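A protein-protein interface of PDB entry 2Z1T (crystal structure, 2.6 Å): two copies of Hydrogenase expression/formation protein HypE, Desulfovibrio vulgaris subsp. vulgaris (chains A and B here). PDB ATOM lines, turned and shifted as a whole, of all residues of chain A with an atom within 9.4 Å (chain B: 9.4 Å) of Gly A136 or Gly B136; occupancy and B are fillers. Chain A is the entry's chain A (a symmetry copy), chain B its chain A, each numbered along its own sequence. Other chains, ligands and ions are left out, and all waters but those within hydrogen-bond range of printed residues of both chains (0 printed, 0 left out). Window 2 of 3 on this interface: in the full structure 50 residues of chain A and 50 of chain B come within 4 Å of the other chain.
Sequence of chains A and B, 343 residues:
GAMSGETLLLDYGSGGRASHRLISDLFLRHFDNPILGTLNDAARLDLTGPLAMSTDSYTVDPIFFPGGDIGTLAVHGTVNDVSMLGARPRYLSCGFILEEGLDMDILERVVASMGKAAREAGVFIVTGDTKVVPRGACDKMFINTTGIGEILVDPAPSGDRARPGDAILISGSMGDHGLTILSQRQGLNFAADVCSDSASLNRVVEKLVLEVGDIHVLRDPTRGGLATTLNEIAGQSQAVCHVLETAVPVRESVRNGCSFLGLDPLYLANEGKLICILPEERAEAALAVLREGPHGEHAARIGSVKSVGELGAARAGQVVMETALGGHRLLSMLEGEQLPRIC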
ATOM      1  N   LEU A  98      -0.881  13.241   0.768  1.00  0.00           N
ATOM      2  CA  LEU A  98      -1.509  12.117   0.081  1.00  0.00           C
ATOM      3  C   LEU A  98      -1.355  12.221  -1.423  1.00  0.00           C
ATOM      4  O   LEU A  98      -1.348  13.324  -1.978  1.00  0.00           O
ATOM      5  CB  LEU A  98      -3.008  12.059   0.389  1.00  0.00           C
ATOM      6  CG  LEU A  98      -3.539  12.341   1.791  1.00  0.00           C
ATOM      7  CD1 LEU A  98      -5.015  12.723   1.714  1.00  0.00           C
ATOM      8  CD2 LEU A  98      -3.328  11.154   2.703  1.00  0.00           C
ATOM      9  N   GLU A  99      -1.271  11.062  -2.072  1.00  0.00           N
ATOM     10  CA  GLU A  99      -1.189  10.969  -3.525  1.00  0.00           C
ATOM     11  C   GLU A  99      -2.578  10.963  -4.173  1.00  0.00           C
ATOM     12  O   GLU A  99      -3.487  10.263  -3.718  1.00  0.00           O
ATOM     13  CB  GLU A  99      -0.415   9.717  -3.931  1.00  0.00           C
ATOM     14  CG  GLU A  99       0.066   9.707  -5.363  1.00  0.00           C
ATOM     15  CD  GLU A  99       0.851   8.451  -5.704  1.00  0.00           C
ATOM     16  OE1 GLU A  99       1.799   8.536  -6.520  1.00  0.00           O
ATOM     17  OE2 GLU A  99       0.529   7.369  -5.161  1.00  0.00           O
ATOM     18  N   GLU A 100      -2.711  11.753  -5.239  1.00  0.00           N
ATOM     19  CA  GLU A 100      -3.928  11.858  -6.048  1.00  0.00           C
ATOM     20  C   GLU A 100      -4.399  10.472  -6.482  1.00  0.00           C
ATOM     21  O   GLU A 100      -3.599   9.668  -6.953  1.00  0.00           O
ATOM     22  CB  GLU A 100      -3.616  12.722  -7.275  1.00  0.00           C
ATOM     23  CG  GLU A 100      -4.782  13.074  -8.192  1.00  0.00           C
ATOM     24  CD  GLU A 100      -4.312  13.394  -9.617  1.00  0.00           C
ATOM     25  OE1 GLU A 100      -5.077  14.042 -10.378  1.00  0.00           O
ATOM     26  OE2 GLU A 100      -3.172  12.998  -9.973  1.00  0.00           O
ATOM     27  N   GLY A 101      -5.688  10.187  -6.297  1.00  0.00           N
ATOM     28  CA  GLY A 101      -6.262   8.894  -6.693  1.00  0.00           C
ATOM     29  C   GLY A 101      -5.905   7.720  -5.786  1.00  0.00           C
ATOM     30  O   GLY A 101      -6.267   6.570  -6.063  1.00  0.00           O
ATOM     31  N   VAL A 133      -1.269  15.768  -3.677  1.00  0.00           N
ATOM     32  CA  VAL A 133      -0.307  16.078  -4.726  1.00  0.00           C
ATOM     33  C   VAL A 133      -0.511  15.198  -5.950  1.00  0.00           C
ATOM     34  O   VAL A 133      -0.987  14.067  -5.820  1.00  0.00           O
ATOM     35  CB  VAL A 133       1.155  15.995  -4.223  1.00  0.00           C
ATOM     36  CG1 VAL A 133       1.424  17.075  -3.178  1.00  0.00           C
ATOM     37  CG2 VAL A 133       1.468  14.612  -3.700  1.00  0.00           C
ATOM     38  N   PRO A 134      -0.186  15.722  -7.150  1.00  0.00           N
ATOM     39  CA  PRO A 134      -0.312  14.911  -8.356  1.00  0.00           C
ATOM     40  C   PRO A 134       0.420  13.564  -8.246  1.00  0.00           C
ATOM     41  O   PRO A 134       1.298  13.388  -7.388  1.00  0.00           O
ATOM     42  CB  PRO A 134       0.303  15.804  -9.448  1.00  0.00           C
ATOM     43  CG  PRO A 134       1.020  16.920  -8.712  1.00  0.00           C
ATOM     44  CD  PRO A 134       0.260  17.092  -7.463  1.00  0.00           C
ATOM     45  N   ARG A 135       0.043  12.613  -9.094  1.00  0.00           N
ATOM     46  CA  ARG A 135       0.637  11.276  -9.025  1.00  0.00           C
ATOM     47  C   ARG A 135       2.093  11.354  -9.461  1.00  0.00           C
ATOM     48  O   ARG A 135       2.436  12.131 -10.359  1.00  0.00           O
ATOM     49  CB  ARG A 135      -0.177  10.277  -9.839  1.00  0.00           C
ATOM     50  CG  ARG A 135      -1.625  10.184  -9.350  1.00  0.00           C
ATOM     51  CD  ARG A 135      -2.515   9.237 -10.161  1.00  0.00           C
ATOM     52  NE  ARG A 135      -2.608   9.633 -11.561  1.00  0.00           N
ATOM     53  CZ  ARG A 135      -2.401   8.811 -12.584  1.00  0.00           C
ATOM     54  NH1 ARG A 135      -2.123   7.526 -12.369  1.00  0.00           N
ATOM     55  NH2 ARG A 135      -2.501   9.268 -13.829  1.00  0.00           N
ATOM     56  N   GLY A 136       2.950  10.593  -8.784  1.00  0.00           N
ATOM     57  CA  GLY A 136       4.396  10.717  -8.956  1.00  0.00           C
ATOM     58  C   GLY A 136       5.043  11.637  -7.932  1.00  0.00           C
ATOM     59  O   GLY A 136       6.107  11.317  -7.393  1.00  0.00           O
ATOM     60  N   ALA A 137       4.403  12.776  -7.662  1.00  0.00           N
ATOM     61  CA  ALA A 137       4.901  13.746  -6.675  1.00  0.00           C
ATOM     62  C   ALA A 137       5.132  13.180  -5.261  1.00  0.00           C
ATOM     63  O   ALA A 137       6.029  13.644  -4.545  1.00  0.00           O
ATOM     64  CB  ALA A 137       3.990  14.961  -6.615  1.00  0.00           C
ATOM     65  N   CYS A 138       4.315  12.208  -4.851  1.00  0.00           N
ATOM     66  CA  CYS A 138       4.578  11.448  -3.619  1.00  0.00           C
ATOM     67  C   CYS A 138       4.074  10.002  -3.711  1.00  0.00           C
ATOM     68  O   CYS A 138       3.166   9.714  -4.497  1.00  0.00           O
ATOM     69  CB  CYS A 138       4.027  12.168  -2.379  1.00  0.00           C
ATOM     70  SG  CYS A 138       2.652  11.369  -1.549  1.00  0.00           S
ATOM     71  N   ASP A 139       4.668   9.107  -2.912  1.00  0.00           N
ATOM     72  CA  ASP A 139       4.355   7.670  -2.956  1.00  0.00           C
ATOM     73  C   ASP A 139       3.234   7.274  -1.995  1.00  0.00           C
ATOM     74  O   ASP A 139       3.475   6.861  -0.862  1.00  0.00           O
ATOM     75  CB  ASP A 139       5.617   6.827  -2.725  1.00  0.00           C
ATOM     76  CG  ASP A 139       5.368   5.313  -2.845  1.00  0.00           C
ATOM     77  OD1 ASP A 139       4.360   4.860  -3.445  1.00  0.00           O
ATOM     78  OD2 ASP A 139       6.213   4.561  -2.332  1.00  0.00           O
ATOM     79  N   LYS A 140       2.007   7.403  -2.492  1.00  0.00           N
ATOM     80  CA  LYS A 140       0.777   7.003  -1.797  1.00  0.00           C
ATOM     81  C   LYS A 140       0.374   7.972  -0.673  1.00  0.00           C
ATOM     82  O   LYS A 140      -0.664   8.635  -0.794  1.00  0.00           O
ATOM     83  CB  LYS A 140       0.802   5.520  -1.356  1.00  0.00           C
ATOM     84  CG  LYS A 140       1.415   4.554  -2.412  1.00  0.00           C
ATOM     85  CD  LYS A 140       0.844   3.121  -2.390  1.00  0.00           C
ATOM     86  CE  LYS A 140       1.283   2.288  -1.168  1.00  0.00           C
ATOM     87  NZ  LYS A 140       2.725   1.889  -1.174  1.00  0.00           N
ATOM     88  N   PHE A 142       2.277  10.261   3.174  1.00  0.00           N
ATOM     89  CA  PHE A 142       3.238  10.482   4.238  1.00  0.00           C
ATOM     90  C   PHE A 142       2.511  11.215   5.345  1.00  0.00           C
ATOM     91  O   PHE A 142       1.562  11.944   5.080  1.00  0.00           O
ATOM     92  CB  PHE A 142       4.363  11.389   3.773  1.00  0.00           C
ATOM     93  CG  PHE A 142       5.210  10.826   2.677  1.00  0.00           C
ATOM     94  CD1 PHE A 142       5.753  11.672   1.722  1.00  0.00           C
ATOM     95  CD2 PHE A 142       5.491   9.473   2.605  1.00  0.00           C
ATOM     96  CE1 PHE A 142       6.543  11.180   0.710  1.00  0.00           C
ATOM     97  CE2 PHE A 142       6.284   8.973   1.594  1.00  0.00           C
ATOM     98  CZ  PHE A 142       6.817   9.829   0.648  1.00  0.00           C
ATOM     99  N   ARG A 341      13.040   4.214   4.321  1.00  0.00           N
ATOM    100  CA  ARG A 341      11.602   4.059   4.564  1.00  0.00           C
ATOM    101  C   ARG A 341      11.175   2.921   5.520  1.00  0.00           C
ATOM    102  O   ARG A 341      10.176   2.245   5.276  1.00  0.00           O
ATOM    103  CB  ARG A 341      10.854   3.979   3.225  1.00  0.00           C
ATOM    104  CG  ARG A 341      10.980   5.242   2.378  1.00  0.00           C
ATOM    105  CD  ARG A 341      10.136   5.171   1.122  1.00  0.00           C
ATOM    106  NE  ARG A 341       8.710   5.226   1.418  1.00  0.00           N
ATOM    107  CZ  ARG A 341       7.747   5.254   0.499  1.00  0.00           C
ATOM    108  NH1 ARG A 341       8.048   5.232  -0.790  1.00  0.00           N
ATOM    109  NH2 ARG A 341       6.477   5.311   0.873  1.00  0.00           N
ATOM    110  N   LEU B  98      12.691  14.717   2.150  1.00  0.00           N
ATOM    111  CA  LEU B  98      13.585  15.071   1.052  1.00  0.00           C
ATOM    112  C   LEU B  98      13.796  13.910   0.101  1.00  0.00           C
ATOM    113  O   LEU B  98      13.809  12.749   0.523  1.00  0.00           O
ATOM    114  CB  LEU B  98      14.959  15.491   1.581  1.00  0.00           C
ATOM    115  CG  LEU B  98      15.096  16.352   2.832  1.00  0.00           C
ATOM    116  CD1 LEU B  98      16.496  16.190   3.418  1.00  0.00           C
ATOM    117  CD2 LEU B  98      14.795  17.802   2.532  1.00  0.00           C
ATOM    118  N   GLU B  99      13.998  14.240  -1.173  1.00  0.00           N
ATOM    119  CA  GLU B  99      14.286  13.259  -2.211  1.00  0.00           C
ATOM    120  C   GLU B  99      15.784  12.949  -2.299  1.00  0.00           C
ATOM    121  O   GLU B  99      16.622  13.855  -2.276  1.00  0.00           O
ATOM    122  CB  GLU B  99      13.773  13.755  -3.561  1.00  0.00           C
ATOM    123  CG  GLU B  99      13.662  12.689  -4.627  1.00  0.00           C
ATOM    124  CD  GLU B  99      13.123  13.232  -5.940  1.00  0.00           C
ATOM    125  OE1 GLU B  99      12.402  12.490  -6.648  1.00  0.00           O
ATOM    126  OE2 GLU B  99      13.415  14.404  -6.276  1.00  0.00           O
ATOM    127  N   GLU B 100      16.091  11.655  -2.402  1.00  0.00           N
ATOM    128  CA  GLU B 100      17.450  11.134  -2.559  1.00  0.00           C
ATOM    129  C   GLU B 100      18.160  11.834  -3.716  1.00  0.00           C
ATOM    130  O   GLU B 100      17.589  11.970  -4.795  1.00  0.00           O
ATOM    131  CB  GLU B 100      17.361   9.627  -2.823  1.00  0.00           C
ATOM    132  CG  GLU B 100      18.673   8.852  -2.886  1.00  0.00           C
ATOM    133  CD  GLU B 100      18.536   7.564  -3.708  1.00  0.00           C
ATOM    134  OE1 GLU B 100      19.392   6.653  -3.557  1.00  0.00           O
ATOM    135  OE2 GLU B 100      17.568   7.463  -4.505  1.00  0.00           O
ATOM    136  N   GLY B 101      19.385  12.300  -3.481  1.00  0.00           N
ATOM    137  CA  GLY B 101      20.174  12.973  -4.522  1.00  0.00           C
ATOM    138  C   GLY B 101      19.731  14.396  -4.853  1.00  0.00           C
ATOM    139  O   GLY B 101      20.269  15.033  -5.765  1.00  0.00           O
ATOM    140  N   VAL B 133      13.891   9.837   1.132  1.00  0.00           N
ATOM    141  CA  VAL B 133      13.190   8.771   0.428  1.00  0.00           C
ATOM    142  C   VAL B 133      13.781   8.528  -0.952  1.00  0.00           C
ATOM    143  O   VAL B 133      14.328   9.455  -1.556  1.00  0.00           O
ATOM    144  CB  VAL B 133      11.666   9.032   0.340  1.00  0.00           C
ATOM    145  CG1 VAL B 133      11.035   9.001   1.730  1.00  0.00           C
ATOM    146  CG2 VAL B 133      11.383  10.330  -0.382  1.00  0.00           C
ATOM    147  N   PRO B 134      13.707   7.275  -1.445  1.00  0.00           N
ATOM    148  CA  PRO B 134      14.212   6.989  -2.783  1.00  0.00           C
ATOM    149  C   PRO B 134      13.623   7.923  -3.852  1.00  0.00           C
ATOM    150  O   PRO B 134      12.584   8.564  -3.632  1.00  0.00           O
ATOM    151  CB  PRO B 134      13.794   5.526  -3.014  1.00  0.00           C
ATOM    152  CG  PRO B 134      12.803   5.203  -1.912  1.00  0.00           C
ATOM    153  CD  PRO B 134      13.210   6.056  -0.782  1.00  0.00           C
ATOM    154  N   ARG B 135      14.296   8.017  -4.995  1.00  0.00           N
ATOM    155  CA  ARG B 135      13.848   8.929  -6.049  1.00  0.00           C
ATOM    156  C   ARG B 135      12.543   8.409  -6.638  1.00  0.00           C
ATOM    157  O   ARG B 135      12.352   7.193  -6.758  1.00  0.00           O
ATOM    158  CB  ARG B 135      14.939   9.126  -7.096  1.00  0.00           C
ATOM    159  CG  ARG B 135      16.223   9.692  -6.486  1.00  0.00           C
ATOM    160  CD  ARG B 135      17.380   9.864  -7.474  1.00  0.00           C
ATOM    161  NE  ARG B 135      17.773   8.601  -8.087  1.00  0.00           N
ATOM    162  CZ  ARG B 135      17.913   8.418  -9.396  1.00  0.00           C
ATOM    163  NH1 ARG B 135      17.727   9.432 -10.240  1.00  0.00           N
ATOM    164  NH2 ARG B 135      18.267   7.224  -9.861  1.00  0.00           N
ATOM    165  N   GLY B 136      11.633   9.328  -6.948  1.00  0.00           N
ATOM    166  CA  GLY B 136      10.269   8.966  -7.329  1.00  0.00           C
ATOM    167  C   GLY B 136       9.296   8.991  -6.160  1.00  0.00           C
ATOM    168  O   GLY B 136       8.172   9.484  -6.297  1.00  0.00           O
ATOM    169  N   ALA B 137       9.725   8.463  -5.011  1.00  0.00           N
ATOM    170  CA  ALA B 137       8.899   8.443  -3.795  1.00  0.00           C
ATOM    171  C   ALA B 137       8.389   9.819  -3.328  1.00  0.00           C
ATOM    172  O   ALA B 137       7.299   9.914  -2.748  1.00  0.00           O
ATOM    173  CB  ALA B 137       9.633   7.740  -2.665  1.00  0.00           C
ATOM    174  N   CYS B 138       9.178  10.872  -3.552  1.00  0.00           N
ATOM    175  CA  CYS B 138       8.702  12.249  -3.351  1.00  0.00           C
ATOM    176  C   CYS B 138       9.364  13.238  -4.319  1.00  0.00           C
ATOM    177  O   CYS B 138      10.463  12.973  -4.817  1.00  0.00           O
ATOM    178  CB  CYS B 138       8.852  12.694  -1.888  1.00  0.00           C
ATOM    179  SG  CYS B 138      10.057  13.985  -1.576  1.00  0.00           S
ATOM    180  N   ASP B 139       8.690  14.365  -4.580  1.00  0.00           N
ATOM    181  CA  ASP B 139       9.154  15.362  -5.558  1.00  0.00           C
ATOM    182  C   ASP B 139      10.040  16.441  -4.934  1.00  0.00           C
ATOM    183  O   ASP B 139       9.574  17.510  -4.545  1.00  0.00           O
ATOM    184  CB  ASP B 139       7.972  15.977  -6.318  1.00  0.00           C
ATOM    185  CG  ASP B 139       8.401  16.966  -7.416  1.00  0.00           C
ATOM    186  OD1 ASP B 139       9.568  16.958  -7.884  1.00  0.00           O
ATOM    187  OD2 ASP B 139       7.541  17.764  -7.823  1.00  0.00           O
ATOM    188  N   LYS B 140      11.331  16.127  -4.866  1.00  0.00           N
ATOM    189  CA  LYS B 140      12.387  17.031  -4.392  1.00  0.00           C
ATOM    190  C   LYS B 140      12.396  17.204  -2.864  1.00  0.00           C
ATOM    191  O   LYS B 140      13.356  16.769  -2.215  1.00  0.00           O
ATOM    192  CB  LYS B 140      12.411  18.369  -5.168  1.00  0.00           C
ATOM    193  CG  LYS B 140      12.183  18.220  -6.701  1.00  0.00           C
ATOM    194  CD  LYS B 140      12.880  19.288  -7.567  1.00  0.00           C
ATOM    195  CE  LYS B 140      12.245  20.691  -7.469  1.00  0.00           C
ATOM    196  NZ  LYS B 140      10.900  20.810  -8.112  1.00  0.00           N
ATOM    197  N   PHE B 142       9.374  18.163   0.824  1.00  0.00           N
ATOM    198  CA  PHE B 142       8.162  18.666   1.443  1.00  0.00           C
ATOM    199  C   PHE B 142       8.512  19.026   2.872  1.00  0.00           C
ATOM    200  O   PHE B 142       9.415  18.433   3.451  1.00  0.00           O
ATOM    201  CB  PHE B 142       7.096  17.588   1.508  1.00  0.00           C
ATOM    202  CG  PHE B 142       6.610  17.105   0.179  1.00  0.00           C
ATOM    203  CD1 PHE B 142       6.232  15.780   0.022  1.00  0.00           C
ATOM    204  CD2 PHE B 142       6.500  17.961  -0.903  1.00  0.00           C
ATOM    205  CE1 PHE B 142       5.772  15.315  -1.186  1.00  0.00           C
ATOM    206  CE2 PHE B 142       6.038  17.502  -2.118  1.00  0.00           C
ATOM    207  CZ  PHE B 142       5.666  16.178  -2.258  1.00  0.00           C
ATOM    208  N   ARG B 341      -0.638  22.027  -5.388  1.00  0.00           N
ATOM    209  CA  ARG B 341       0.704  22.460  -4.985  1.00  0.00           C
ATOM    210  C   ARG B 341       1.001  23.975  -5.066  1.00  0.00           C
ATOM    211  O   ARG B 341       2.095  24.376  -5.461  1.00  0.00           O
ATOM    212  CB  ARG B 341       1.765  21.639  -5.736  1.00  0.00           C
ATOM    213  CG  ARG B 341       1.717  20.147  -5.422  1.00  0.00           C
ATOM    214  CD  ARG B 341       2.846  19.390  -6.088  1.00  0.00           C
ATOM    215  NE  ARG B 341       4.142  19.714  -5.505  1.00  0.00           N
ATOM    216  CZ  ARG B 341       5.292  19.140  -5.850  1.00  0.00           C
ATOM    217  NH1 ARG B 341       5.323  18.204  -6.786  1.00  0.00           N
ATOM    218  NH2 ARG B 341       6.418  19.503  -5.251  1.00  0.00           N
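Gly A136 touches just one residue of chain B: Gly B136. Of chain A, only Gly A136 comes within 4 Å of Gly B136. Ala A137 touches four residues of chain B. Of chain A, only Cys A138 (3.2 Å), Asp A139 (2.8 Å), Phe A142 (3.4 Å) and Arg A341 (3.5 Å) come within 4 Å of Ala B137. Printed residues of chain B within 4 Å of Arg A341: Val B133 (3.8 Å), Pro B134 (3.7 Å) and Ala B137 (3.5 Å). Of the printed residues of chain A, Phe B142 touches Ala A137 and Cys A138. Printed residues of chain A within 4 Å of Asp B139: Ala A137 (2.8 Å). Printed residues of chain B within 4 Å of Asp A139: Ala B137. Lys B140 touches none of the printed residues of chain A. The nearest printed residue of chain A that does not touch Gly B136 is Cys A138 (4.9 Å). The nearest printed residue of chain A that does not touch Phe B142 is Val A133 (4.4 Å).
The backbone carbonyl oxygen (O) of Val A133 is in hydrogen-bond range of the backbone NH (N) of Glu A100, 2.9 Å away. The backbone carbonyl oxygen of Val B133 is in hydrogen-bond range of the backbone NH of Glu B100 (2.9 Å). N of Val A133 lies within hydrogen-bond range of O of Leu A98 (3.0 Å). The backbone NH (N) of Val B133 lies within hydrogen-bond range of the backbone carbonyl oxygen (O) of Leu B98 (3.0 Å). OE1 of Glu B99 lies within hydrogen-bond range of N of Gly B136 (3.3 Å). The backbone NH (N) of Gly A136 lies within hydrogen-bond range of the side-chain carboxylate (OE1) of Glu A99, 3.3 Å away.
Arg B341 touches Val A133. CD of Pro A134 touches CD of Arg B341, 3.7 Å away. Cys B138 touches Ala A137 (CA to O, 3.2 Å). NH1 of Arg B341 touches CB of Ala A137 (3.5 Å). Cys A138 touches Ala B137 (CA to O, 3.2 Å). Cys A138 touches Phe B142 (CB to CE1, 3.8 Å). Phe A142 touches Ala B137. CE1 of Phe A142 touches CB of Cys B138 (3.8 Å). Val B133 touches Arg A341. Ala B137 touches Arg A341 (CB to NH1, 3.5 Å).
Val A133 touches Arg B341, and with the chains exchanged Arg A341 touches Val B133. Pro A134 touches Arg B341, and with the chains exchanged Arg A341 touches Pro B134. Ala A137 touches Asp B139, and with the chains exchanged Asp A139 touches Ala B137. Ala A137 touches Phe B142, and with the chains exchanged Phe A142 touches Ala B137. 14 positions are printed for both chains.
Printed residues of chain B that touch a printed residue of chain A: Val B133, Pro B134, Gly B136, Ala B137, Cys B138, Asp B139, Phe B142 and Arg B341. Hydrophobic or aromatic side chains of chain B that line the printed part of chain A: Val B133, Pro B134, Ala B137 and Phe B142. Of the 14 printed residues of chain A, 8 touch a printed residue of chain B. Hydrophobic or aromatic side chains of chain A that line the printed part of chain B: Val A133, Pro A134, Ala A137 and Phe A142.
The backbone carbonyl oxygen of Gly A136 sits close to the backbone carbonyl oxygen of Gly B136, 3.0 Å away. The backbone carbonyl oxygen (O) of Ala B137 lies within hydrogen-bond range of the backbone NH (N) of Asp A139, at 2.8 Å. O of Ala A137 lies within hydrogen-bond range of N of Asp B139 (2.8 Å).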
